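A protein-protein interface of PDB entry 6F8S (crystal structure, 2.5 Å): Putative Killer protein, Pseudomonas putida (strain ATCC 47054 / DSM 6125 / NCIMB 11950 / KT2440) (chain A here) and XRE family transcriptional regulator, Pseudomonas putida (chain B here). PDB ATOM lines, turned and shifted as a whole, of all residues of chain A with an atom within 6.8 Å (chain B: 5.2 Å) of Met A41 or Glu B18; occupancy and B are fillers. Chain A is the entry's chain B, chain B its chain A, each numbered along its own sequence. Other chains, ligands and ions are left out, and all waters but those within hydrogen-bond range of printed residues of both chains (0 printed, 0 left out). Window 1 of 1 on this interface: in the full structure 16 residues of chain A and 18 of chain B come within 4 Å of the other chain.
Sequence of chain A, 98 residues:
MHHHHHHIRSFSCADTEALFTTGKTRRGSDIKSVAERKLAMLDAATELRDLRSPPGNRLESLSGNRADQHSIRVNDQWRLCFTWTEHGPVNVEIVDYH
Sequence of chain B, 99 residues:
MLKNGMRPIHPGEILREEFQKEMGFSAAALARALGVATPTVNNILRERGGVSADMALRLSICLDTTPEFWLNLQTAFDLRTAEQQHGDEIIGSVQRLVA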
ATOM      1  N   VAL A  34      11.045  29.658  26.335  1.00  0.00           N
ATOM      2  CA  VAL A  34       9.685  29.412  25.873  1.00  0.00           C
ATOM      3  C   VAL A  34       9.475  27.910  25.650  1.00  0.00           C
ATOM      4  O   VAL A  34       8.456  27.343  26.057  1.00  0.00           O
ATOM      5  CB  VAL A  34       9.390  30.204  24.573  1.00  0.00           C
ATOM      6  CG1 VAL A  34       8.049  29.774  23.945  1.00  0.00           C
ATOM      7  CG2 VAL A  34       9.401  31.698  24.856  1.00  0.00           C
ATOM      8  N   GLU A  36      11.020  25.522  27.102  1.00  0.00           N
ATOM      9  CA  GLU A  36      11.029  24.872  28.394  1.00  0.00           C
ATOM     10  C   GLU A  36       9.678  24.938  29.036  1.00  0.00           C
ATOM     11  O   GLU A  36       9.264  24.028  29.723  1.00  0.00           O
ATOM     12  CB  GLU A  36      12.052  25.528  29.293  1.00  0.00           C
ATOM     13  CG  GLU A  36      13.456  25.203  28.840  1.00  0.00           C
ATOM     14  CD  GLU A  36      14.505  25.911  29.648  1.00  0.00           C
ATOM     15  OE1 GLU A  36      14.304  27.122  29.934  1.00  0.00           O
ATOM     16  OE2 GLU A  36      15.511  25.259  29.989  1.00  0.00           O
ATOM     17  N   ARG A  37       9.019  26.058  28.802  1.00  0.00           N
ATOM     18  CA  ARG A  37       7.728  26.326  29.347  1.00  0.00           C
ATOM     19  C   ARG A  37       6.653  25.492  28.645  1.00  0.00           C
ATOM     20  O   ARG A  37       5.726  24.967  29.292  1.00  0.00           O
ATOM     21  CB  ARG A  37       7.434  27.811  29.225  1.00  0.00           C
ATOM     22  CG  ARG A  37       6.155  28.228  29.897  1.00  0.00           C
ATOM     23  CD  ARG A  37       6.114  29.737  30.129  1.00  0.00           C
ATOM     24  NE  ARG A  37       6.124  30.466  28.867  1.00  0.00           N
ATOM     25  CZ  ARG A  37       7.030  31.382  28.537  1.00  0.00           C
ATOM     26  NH1 ARG A  37       7.995  31.687  29.389  1.00  0.00           N
ATOM     27  NH2 ARG A  37       6.964  31.999  27.362  1.00  0.00           N
ATOM     28  N   LYS A  38       6.773  25.375  27.321  1.00  0.00           N
ATOM     29  CA  LYS A  38       5.840  24.565  26.534  1.00  0.00           C
ATOM     30  C   LYS A  38       5.959  23.100  26.936  1.00  0.00           C
ATOM     31  O   LYS A  38       4.932  22.419  27.152  1.00  0.00           O
ATOM     32  CB  LYS A  38       6.099  24.736  25.030  1.00  0.00           C
ATOM     33  CG  LYS A  38       6.015  26.171  24.552  1.00  0.00           C
ATOM     34  CD  LYS A  38       4.588  26.627  24.420  1.00  0.00           C
ATOM     35  CE  LYS A  38       4.502  28.140  24.329  1.00  0.00           C
ATOM     36  NZ  LYS A  38       3.164  28.586  23.832  1.00  0.00           N
ATOM     37  N   LEU A  39       7.202  22.620  27.051  1.00  0.00           N
ATOM     38  CA  LEU A  39       7.418  21.268  27.564  1.00  0.00           C
ATOM     39  C   LEU A  39       6.812  21.110  28.973  1.00  0.00           C
ATOM     40  O   LEU A  39       6.200  20.085  29.269  1.00  0.00           O
ATOM     41  CB  LEU A  39       8.894  20.911  27.589  1.00  0.00           C
ATOM     42  CG  LEU A  39       9.618  20.753  26.250  1.00  0.00           C
ATOM     43  CD1 LEU A  39      10.974  20.133  26.520  1.00  0.00           C
ATOM     44  CD2 LEU A  39       8.824  19.902  25.273  1.00  0.00           C
ATOM     45  N   ALA A  40       6.963  22.120  29.827  1.00  0.00           N
ATOM     46  CA  ALA A  40       6.348  22.097  31.160  1.00  0.00           C
ATOM     47  C   ALA A  40       4.831  21.887  31.090  1.00  0.00           C
ATOM     48  O   ALA A  40       4.268  21.057  31.793  1.00  0.00           O
ATOM     49  CB  ALA A  40       6.651  23.402  31.910  1.00  0.00           C
ATOM     50  N   MET A  41       4.173  22.659  30.235  1.00  0.00           N
ATOM     51  CA  MET A  41       2.730  22.593  30.109  1.00  0.00           C
ATOM     52  C   MET A  41       2.293  21.241  29.576  1.00  0.00           C
ATOM     53  O   MET A  41       1.348  20.647  30.116  1.00  0.00           O
ATOM     54  CB  MET A  41       2.220  23.717  29.215  1.00  0.00           C
ATOM     55  CG  MET A  41       2.471  25.075  29.811  1.00  0.00           C
ATOM     56  SD  MET A  41       1.664  26.396  28.898  1.00  0.00           S
ATOM     57  CE  MET A  41       2.512  26.288  27.331  1.00  0.00           C
ATOM     58  N   LEU A  42       2.988  20.756  28.541  1.00  0.00           N
ATOM     59  CA  LEU A  42       2.709  19.440  27.961  1.00  0.00           C
ATOM     60  C   LEU A  42       2.748  18.347  29.017  1.00  0.00           C
ATOM     61  O   LEU A  42       1.849  17.513  29.083  1.00  0.00           O
ATOM     62  CB  LEU A  42       3.712  19.088  26.860  1.00  0.00           C
ATOM     63  CG  LEU A  42       3.497  19.587  25.438  1.00  0.00           C
ATOM     64  CD1 LEU A  42       4.631  19.078  24.613  1.00  0.00           C
ATOM     65  CD2 LEU A  42       2.186  19.086  24.893  1.00  0.00           C
ATOM     66  N   ASP A  43       3.793  18.349  29.838  1.00  0.00           N
ATOM     67  CA  ASP A  43       3.897  17.366  30.899  1.00  0.00           C
ATOM     68  C   ASP A  43       2.808  17.550  31.966  1.00  0.00           C
ATOM     69  O   ASP A  43       2.346  16.574  32.546  1.00  0.00           O
ATOM     70  CB  ASP A  43       5.283  17.416  31.538  1.00  0.00           C
ATOM     71  CG  ASP A  43       6.329  16.675  30.711  1.00  0.00           C
ATOM     72  N   ALA A  44       2.376  18.785  32.204  1.00  0.00           N
ATOM     73  CA  ALA A  44       1.412  19.035  33.261  1.00  0.00           C
ATOM     74  C   ALA A  44      -0.039  18.800  32.806  1.00  0.00           C
ATOM     75  O   ALA A  44      -0.920  18.660  33.632  1.00  0.00           O
ATOM     76  CB  ALA A  44       1.563  20.442  33.773  1.00  0.00           C
ATOM     77  N   ALA A  45      -0.279  18.769  31.498  1.00  0.00           N
ATOM     78  CA  ALA A  45      -1.636  18.714  30.966  1.00  0.00           C
ATOM     79  C   ALA A  45      -2.360  17.426  31.337  1.00  0.00           C
ATOM     80  O   ALA A  45      -1.806  16.326  31.275  1.00  0.00           O
ATOM     81  CB  ALA A  45      -1.622  18.881  29.458  1.00  0.00           C
ATOM     82  N   THR A  46      -3.616  17.589  31.721  1.00  0.00           N
ATOM     83  CA  THR A  46      -4.460  16.484  32.129  1.00  0.00           C
ATOM     84  C   THR A  46      -5.562  16.262  31.100  1.00  0.00           C
ATOM     85  O   THR A  46      -6.023  15.148  30.898  1.00  0.00           O
ATOM     86  CB  THR A  46      -5.028  16.767  33.512  1.00  0.00           C
ATOM     87  OG1 THR A  46      -4.117  16.244  34.478  1.00  0.00           O
ATOM     88  CG2 THR A  46      -6.346  16.157  33.700  1.00  0.00           C
ATOM     89  N   ASP A  50      -6.220  21.968  28.488  1.00  0.00           N
ATOM     90  CA  ASP A  50      -5.047  22.530  29.111  1.00  0.00           C
ATOM     91  C   ASP A  50      -4.081  23.058  28.056  1.00  0.00           C
ATOM     92  O   ASP A  50      -3.323  23.998  28.318  1.00  0.00           O
ATOM     93  CB  ASP A  50      -4.363  21.492  30.001  1.00  0.00           C
ATOM     94  CG  ASP A  50      -5.219  21.114  31.220  1.00  0.00           C
ATOM     95  OD1 ASP A  50      -6.016  21.973  31.674  1.00  0.00           O
ATOM     96  OD2 ASP A  50      -5.084  19.973  31.734  1.00  0.00           O
ATOM     97  N   LEU A  51      -4.105  22.475  26.858  1.00  0.00           N
ATOM     98  CA  LEU A  51      -3.213  22.944  25.797  1.00  0.00           C
ATOM     99  C   LEU A  51      -3.934  23.865  24.833  1.00  0.00           C
ATOM    100  O   LEU A  51      -3.326  24.751  24.267  1.00  0.00           O
ATOM    101  CB  LEU A  51      -2.601  21.767  25.056  1.00  0.00           C
ATOM    102  CG  LEU A  51      -1.728  20.947  26.006  1.00  0.00           C
ATOM    103  CD1 LEU A  51      -1.335  19.650  25.341  1.00  0.00           C
ATOM    104  CD2 LEU A  51      -0.484  21.741  26.453  1.00  0.00           C
ATOM    105  N   SER A  53      -6.578  25.927  25.744  1.00  0.00           N
ATOM    106  CA  SER A  53      -7.022  27.172  26.366  1.00  0.00           C
ATOM    107  C   SER A  53      -5.988  28.300  26.372  1.00  0.00           C
ATOM    108  O   SER A  53      -6.360  29.433  26.089  1.00  0.00           O
ATOM    109  CB  SER A  53      -7.508  26.914  27.792  1.00  0.00           C
ATOM    110  OG  SER A  53      -8.742  26.218  27.752  1.00  0.00           O
ATOM    111  N   PRO A  54      -4.706  28.014  26.702  1.00  0.00           N
ATOM    112  CA  PRO A  54      -3.794  29.167  26.756  1.00  0.00           C
ATOM    113  C   PRO A  54      -3.642  29.790  25.380  1.00  0.00           C
ATOM    114  O   PRO A  54      -3.231  29.099  24.451  1.00  0.00           O
ATOM    115  CB  PRO A  54      -2.460  28.560  27.240  1.00  0.00           C
ATOM    116  CG  PRO A  54      -2.817  27.243  27.824  1.00  0.00           C
ATOM    117  CD  PRO A  54      -4.008  26.758  27.034  1.00  0.00           C
ATOM    118  N   PRO A  55      -4.002  31.072  25.232  1.00  0.00           N
ATOM    119  CA  PRO A  55      -3.939  31.652  23.884  1.00  0.00           C
ATOM    120  C   PRO A  55      -2.492  31.704  23.356  1.00  0.00           C
ATOM    121  O   PRO A  55      -2.259  31.667  22.144  1.00  0.00           O
ATOM    122  CB  PRO A  55      -4.535  33.050  24.076  1.00  0.00           C
ATOM    123  CG  PRO A  55      -4.422  33.333  25.545  1.00  0.00           C
ATOM    124  CD  PRO A  55      -4.487  32.026  26.247  1.00  0.00           C
ATOM    125  N   GLY A  56      -1.521  31.749  24.262  1.00  0.00           N
ATOM    126  CA  GLY A  56      -0.125  31.639  23.869  1.00  0.00           C
ATOM    127  C   GLY A  56       0.249  30.339  23.164  1.00  0.00           C
ATOM    128  O   GLY A  56       1.288  30.269  22.521  1.00  0.00           O
ATOM    129  N   ASN A  57      -0.579  29.302  23.289  1.00  0.00           N
ATOM    130  CA  ASN A  57      -0.294  28.039  22.616  1.00  0.00           C
ATOM    131  C   ASN A  57      -0.726  28.050  21.173  1.00  0.00           C
ATOM    132  O   ASN A  57      -0.187  27.288  20.371  1.00  0.00           O
ATOM    133  CB  ASN A  57      -0.973  26.872  23.325  1.00  0.00           C
ATOM    134  CG  ASN A  57      -0.135  26.318  24.441  1.00  0.00           C
ATOM    135  OD1 ASN A  57       0.959  26.814  24.715  1.00  0.00           O
ATOM    136  ND2 ASN A  57      -0.655  25.297  25.122  1.00  0.00           N
ATOM    137  N   ILE A  72       1.358  23.237  19.212  1.00  0.00           N
ATOM    138  CA  ILE A  72       1.335  24.507  19.905  1.00  0.00           C
ATOM    139  C   ILE A  72       2.494  25.376  19.432  1.00  0.00           C
ATOM    140  O   ILE A  72       3.576  24.882  19.103  1.00  0.00           O
ATOM    141  CB  ILE A  72       1.375  24.319  21.433  1.00  0.00           C
ATOM    142  CG1 ILE A  72       2.583  23.504  21.845  1.00  0.00           C
ATOM    143  CG2 ILE A  72       0.080  23.629  21.946  1.00  0.00           C
ATOM    144  CD1 ILE A  72       2.759  23.437  23.334  1.00  0.00           C
ATOM    145  N   ARG A  73       2.243  26.676  19.356  1.00  0.00           N
ATOM    146  CA  ARG A  73       3.249  27.628  18.928  1.00  0.00           C
ATOM    147  C   ARG A  73       4.372  27.720  19.953  1.00  0.00           C
ATOM    148  O   ARG A  73       4.107  27.882  21.140  1.00  0.00           O
ATOM    149  CB  ARG A  73       2.602  29.001  18.717  1.00  0.00           C
ATOM    150  CG  ARG A  73       3.507  30.081  18.103  1.00  0.00           C
ATOM    151  CD  ARG A  73       2.677  31.288  17.652  1.00  0.00           C
ATOM    152  NE  ARG A  73       3.468  32.301  16.959  1.00  0.00           N
ATOM    153  CZ  ARG A  73       4.210  33.224  17.568  1.00  0.00           C
ATOM    154  NH1 ARG A  73       4.275  33.260  18.894  1.00  0.00           N
ATOM    155  NH2 ARG A  73       4.900  34.107  16.855  1.00  0.00           N
ATOM    156  N   PRO A  89       0.287  13.888  26.477  1.00  0.00           N
ATOM    157  CA  PRO A  89       0.909  14.068  25.157  1.00  0.00           C
ATOM    158  C   PRO A  89       1.838  12.924  24.774  1.00  0.00           C
ATOM    159  O   PRO A  89       2.667  12.521  25.577  1.00  0.00           O
ATOM    160  CB  PRO A  89       1.696  15.367  25.318  1.00  0.00           C
ATOM    161  CG  PRO A  89       0.997  16.094  26.419  1.00  0.00           C
ATOM    162  CD  PRO A  89       0.546  15.025  27.373  1.00  0.00           C
ATOM    163  N   GLU B  13       4.614  31.891  36.015  1.00  0.00           N
ATOM    164  CA  GLU B  13       5.194  32.200  34.706  1.00  0.00           C
ATOM    165  C   GLU B  13       4.208  31.814  33.594  1.00  0.00           C
ATOM    166  O   GLU B  13       4.047  32.544  32.615  1.00  0.00           O
ATOM    167  CB  GLU B  13       6.537  31.488  34.503  1.00  0.00           C
ATOM    168  CG  GLU B  13       7.136  31.631  33.085  1.00  0.00           C
ATOM    169  CD  GLU B  13       8.510  30.982  32.951  1.00  0.00           C
ATOM    170  OE1 GLU B  13       9.202  30.842  33.987  1.00  0.00           O
ATOM    171  OE2 GLU B  13       8.896  30.596  31.817  1.00  0.00           O
ATOM    172  N   ILE B  14       3.549  30.670  33.750  1.00  0.00           N
ATOM    173  CA  ILE B  14       2.534  30.254  32.787  1.00  0.00           C
ATOM    174  C   ILE B  14       1.379  31.246  32.741  1.00  0.00           C
ATOM    175  O   ILE B  14       0.950  31.657  31.663  1.00  0.00           O
ATOM    176  CB  ILE B  14       1.957  28.858  33.119  1.00  0.00           C
ATOM    177  CG1 ILE B  14       3.087  27.875  33.398  1.00  0.00           C
ATOM    178  CG2 ILE B  14       1.058  28.368  31.995  1.00  0.00           C
ATOM    179  CD1 ILE B  14       3.816  27.515  32.193  1.00  0.00           C
ATOM    180  N   LEU B  15       0.860  31.600  33.917  1.00  0.00           N
ATOM    181  CA  LEU B  15      -0.243  32.536  33.997  1.00  0.00           C
ATOM    182  C   LEU B  15       0.153  33.844  33.309  1.00  0.00           C
ATOM    183  O   LEU B  15      -0.592  34.367  32.486  1.00  0.00           O
ATOM    184  CB  LEU B  15      -0.647  32.784  35.452  1.00  0.00           C
ATOM    185  CG  LEU B  15      -1.966  33.537  35.685  1.00  0.00           C
ATOM    186  CD1 LEU B  15      -3.150  32.791  35.081  1.00  0.00           C
ATOM    187  CD2 LEU B  15      -2.215  33.753  37.172  1.00  0.00           C
ATOM    188  N   ARG B  16       1.342  34.346  33.619  1.00  0.00           N
ATOM    189  CA  ARG B  16       1.771  35.627  33.065  1.00  0.00           C
ATOM    190  C   ARG B  16       2.030  35.532  31.568  1.00  0.00           C
ATOM    191  O   ARG B  16       1.449  36.280  30.788  1.00  0.00           O
ATOM    192  CB  ARG B  16       3.023  36.127  33.770  1.00  0.00           C
ATOM    193  CG  ARG B  16       3.345  37.575  33.497  1.00  0.00           C
ATOM    194  CD  ARG B  16       4.804  37.866  33.838  1.00  0.00           C
ATOM    195  NE  ARG B  16       5.228  37.117  35.015  1.00  0.00           N
ATOM    196  CZ  ARG B  16       6.219  36.228  35.027  1.00  0.00           C
ATOM    197  NH1 ARG B  16       6.912  35.976  33.924  1.00  0.00           N
ATOM    198  NH2 ARG B  16       6.511  35.586  36.152  1.00  0.00           N
ATOM    199  N   GLU B  17       2.881  34.590  31.171  1.00  0.00           N
ATOM    200  CA  GLU B  17       3.348  34.522  29.789  1.00  0.00           C
ATOM    201  C   GLU B  17       2.369  33.906  28.818  1.00  0.00           C
ATOM    202  O   GLU B  17       2.327  34.300  27.666  1.00  0.00           O
ATOM    203  CB  GLU B  17       4.661  33.741  29.702  1.00  0.00           C
ATOM    204  CG  GLU B  17       5.787  34.344  30.515  1.00  0.00           C
ATOM    205  CD  GLU B  17       5.908  35.821  30.283  1.00  0.00           C
ATOM    206  OE1 GLU B  17       5.754  36.254  29.116  1.00  0.00           O
ATOM    207  OE2 GLU B  17       6.143  36.552  31.269  1.00  0.00           O
ATOM    208  N   GLU B  18       1.589  32.932  29.269  1.00  0.00           N
ATOM    209  CA  GLU B  18       0.761  32.168  28.348  1.00  0.00           C
ATOM    210  C   GLU B  18      -0.703  32.621  28.357  1.00  0.00           C
ATOM    211  O   GLU B  18      -1.453  32.342  27.416  1.00  0.00           O
ATOM    212  CB  GLU B  18       0.865  30.680  28.679  1.00  0.00           C
ATOM    213  CG  GLU B  18       2.286  30.146  28.686  1.00  0.00           C
ATOM    214  CD  GLU B  18       2.993  30.311  27.351  1.00  0.00           C
ATOM    215  OE1 GLU B  18       2.329  30.199  26.294  1.00  0.00           O
ATOM    216  OE2 GLU B  18       4.222  30.557  27.359  1.00  0.00           O
ATOM    217  N   PHE B  19      -1.113  33.311  29.421  1.00  0.00           N
ATOM    218  CA  PHE B  19      -2.463  33.866  29.474  1.00  0.00           C
ATOM    219  C   PHE B  19      -2.467  35.395  29.478  1.00  0.00           C
ATOM    220  O   PHE B  19      -2.991  36.017  28.544  1.00  0.00           O
ATOM    221  CB  PHE B  19      -3.217  33.353  30.707  1.00  0.00           C
ATOM    222  CG  PHE B  19      -3.752  31.976  30.544  1.00  0.00           C
ATOM    223  CD1 PHE B  19      -3.015  30.883  30.961  1.00  0.00           C
ATOM    224  CD2 PHE B  19      -4.990  31.767  29.967  1.00  0.00           C
ATOM    225  CE1 PHE B  19      -3.511  29.591  30.819  1.00  0.00           C
ATOM    226  CE2 PHE B  19      -5.487  30.488  29.812  1.00  0.00           C
ATOM    227  CZ  PHE B  19      -4.744  29.395  30.241  1.00  0.00           C
ATOM    228  N   GLN B  20      -1.890  35.987  30.525  1.00  0.00           N
ATOM    229  CA  GLN B  20      -2.005  37.425  30.752  1.00  0.00           C
ATOM    230  C   GLN B  20      -1.488  38.266  29.588  1.00  0.00           C
ATOM    231  O   GLN B  20      -2.105  39.267  29.228  1.00  0.00           O
ATOM    232  CB  GLN B  20      -1.267  37.850  32.024  1.00  0.00           C
ATOM    233  CG  GLN B  20      -1.556  39.309  32.382  1.00  0.00           C
ATOM    234  CD  GLN B  20      -0.765  39.814  33.564  1.00  0.00           C
ATOM    235  OE1 GLN B  20       0.436  39.567  33.669  1.00  0.00           O
ATOM    236  NE2 GLN B  20      -1.431  40.540  34.458  1.00  0.00           N
ATOM    237  N   GLU B  22      -1.206  37.678  26.286  1.00  0.00           N
ATOM    238  CA  GLU B  22      -1.972  37.649  25.048  1.00  0.00           C
ATOM    239  C   GLU B  22      -3.384  38.171  25.261  1.00  0.00           C
ATOM    240  O   GLU B  22      -3.976  38.749  24.361  1.00  0.00           O
ATOM    241  CB  GLU B  22      -2.012  36.227  24.479  1.00  0.00           C
ATOM    242  CG  GLU B  22      -0.648  35.552  24.377  1.00  0.00           C
ATOM    243  CD  GLU B  22      -0.154  34.957  25.701  1.00  0.00           C
ATOM    244  OE1 GLU B  22      -0.581  35.415  26.783  1.00  0.00           O
ATOM    245  OE2 GLU B  22       0.671  34.021  25.657  1.00  0.00           O
ATOM    246  N   PHE B  69      -3.849  20.694  36.150  1.00  0.00           N
ATOM    247  CA  PHE B  69      -2.871  21.417  35.350  1.00  0.00           C
ATOM    248  C   PHE B  69      -2.062  22.362  36.244  1.00  0.00           C
ATOM    249  O   PHE B  69      -0.821  22.355  36.227  1.00  0.00           O
ATOM    250  CB  PHE B  69      -3.572  22.197  34.233  1.00  0.00           C
ATOM    251  CG  PHE B  69      -2.639  23.025  33.377  1.00  0.00           C
ATOM    252  CD1 PHE B  69      -1.749  22.409  32.512  1.00  0.00           C
ATOM    253  CD2 PHE B  69      -2.692  24.415  33.417  1.00  0.00           C
ATOM    254  CE1 PHE B  69      -0.898  23.160  31.719  1.00  0.00           C
ATOM    255  CE2 PHE B  69      -1.860  25.174  32.635  1.00  0.00           C
ATOM    256  CZ  PHE B  69      -0.952  24.547  31.772  1.00  0.00           C
ATOM    257  N   LEU B  73       2.000  21.881  37.913  1.00  0.00           N
ATOM    258  CA  LEU B  73       3.060  22.856  37.679  1.00  0.00           C
ATOM    259  C   LEU B  73       3.667  23.255  39.027  1.00  0.00           C
ATOM    260  O   LEU B  73       4.897  23.370  39.167  1.00  0.00           O
ATOM    261  CB  LEU B  73       2.520  24.075  36.923  1.00  0.00           C
ATOM    262  CG  LEU B  73       2.039  23.830  35.484  1.00  0.00           C
ATOM    263  CD1 LEU B  73       1.127  24.982  35.021  1.00  0.00           C
ATOM    264  CD2 LEU B  73       3.182  23.626  34.496  1.00  0.00           C
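The side-chain carboxylate (OE2) of Glu B13 is in salt-bridge range of the guanidinium group (NH1) of Arg A37 (2.8 Å). The side-chain carboxylate (OE2) of Glu B18 lies within salt-bridge range of the guanidinium group (NE) of Arg A37 (2.4 Å). The side-chain carboxylate (OE1) of Glu B18 is in salt-bridge range of the side-chain amino group (NZ) of Lys A38. The backbone NH (N) of Gly A56 lies within hydrogen-bond range of the backbone carbonyl oxygen (O) of Glu B18, at 3.2 Å. N of Gly A56 sits close to OE2 of Glu B22 (3.5 Å).
The backbone carbonyl oxygen of Ile B14 is in hydrogen-bond range of the backbone NH of Phe B19, 3.5 Å away. The guanidinium group of Arg B16 lies within salt-bridge range of the side-chain carboxylate of Glu B17, 2.8 Å away. N of Phe B19 lies close to OE1 of Glu B22, 3.4 Å away. The backbone carbonyl oxygen (O) of Gly A56 lies within hydrogen-bond range of the side-chain amino group (NZ) of Lys A38 (2.8 Å). OD1 of Asn A57 is in hydrogen-bond range of NZ of Lys A38 (3.0 Å). N of Arg A73 sits at hydrogen-bond distance from O of Asn A57, at 2.7 Å.
Among the printed residues, merely in contact across the chains: Pro A55 with Glu B18 (3.3 Å), Arg A37 with Ile B14 (3.4 Å), Arg A37 with Glu B17 (3.5 Å), Asp A50 with Phe B69 (3.5 Å), Pro A54 with Phe B19 (3.6 Å), Ala A44 with Leu B73 (3.6 Å), Met A41 with Ile B14 (3.7 Å), Met A41 with Phe B69 (3.7 Å), Pro A55 with Phe B19 (3.8 Å), Ala A44 with Phe B69 (3.8 Å), Met A41 with Glu B18 (3.8 Å), Ala A40 with Leu B73 (3.9 Å), Pro A55 with Glu B22 (3.9 Å), Pro A54 with Glu B18 (3.9 Å), Ser A53 with Phe B19 (3.97 Å) and Asn A57 with Glu B18 (3.98 Å).
Met A41 touches just these residues of chain B: Ile B14, Glu B18 and Phe B69. Of the printed residues of chain A, Glu B13 touches Arg A37. Of chain A, only Arg A37 (2.4 Å), Lys A38 (3.1 Å), Met A41 (3.8 Å), Pro A54 (3.9 Å), Pro A55 (3.3 Å), Gly A56 (3.2 Å) and Asn A57 (3.98 Å) come within 4 Å of Glu B18. Printed residues of chain A within 4 Å of Leu B73: Ala A40 and Ala A44.
Of the 11 printed residues of chain B, 8 touch a printed residue of chain A. Printed residues of chain B that touch a printed residue of chain A: Glu B13, Ile B14, Glu B17, Glu B18, Phe B19, Glu B22, Phe B69 and Leu B73. Hydrophobic or aromatic side chains of chain A that line the printed part of chain B: Met A41, Ala A44, Pro A54 and Pro A55. Along chain A the printed residues that touch a printed residue of chain B span positions 37 to 57. Among the printed residues, Asp or Glu carboxylates within 4 Å of a Lys or Arg side-chain nitrogen of the other chain: Arg A37 with Glu B13, Arg A37 with Glu B18 and Lys A38 with Glu B18.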
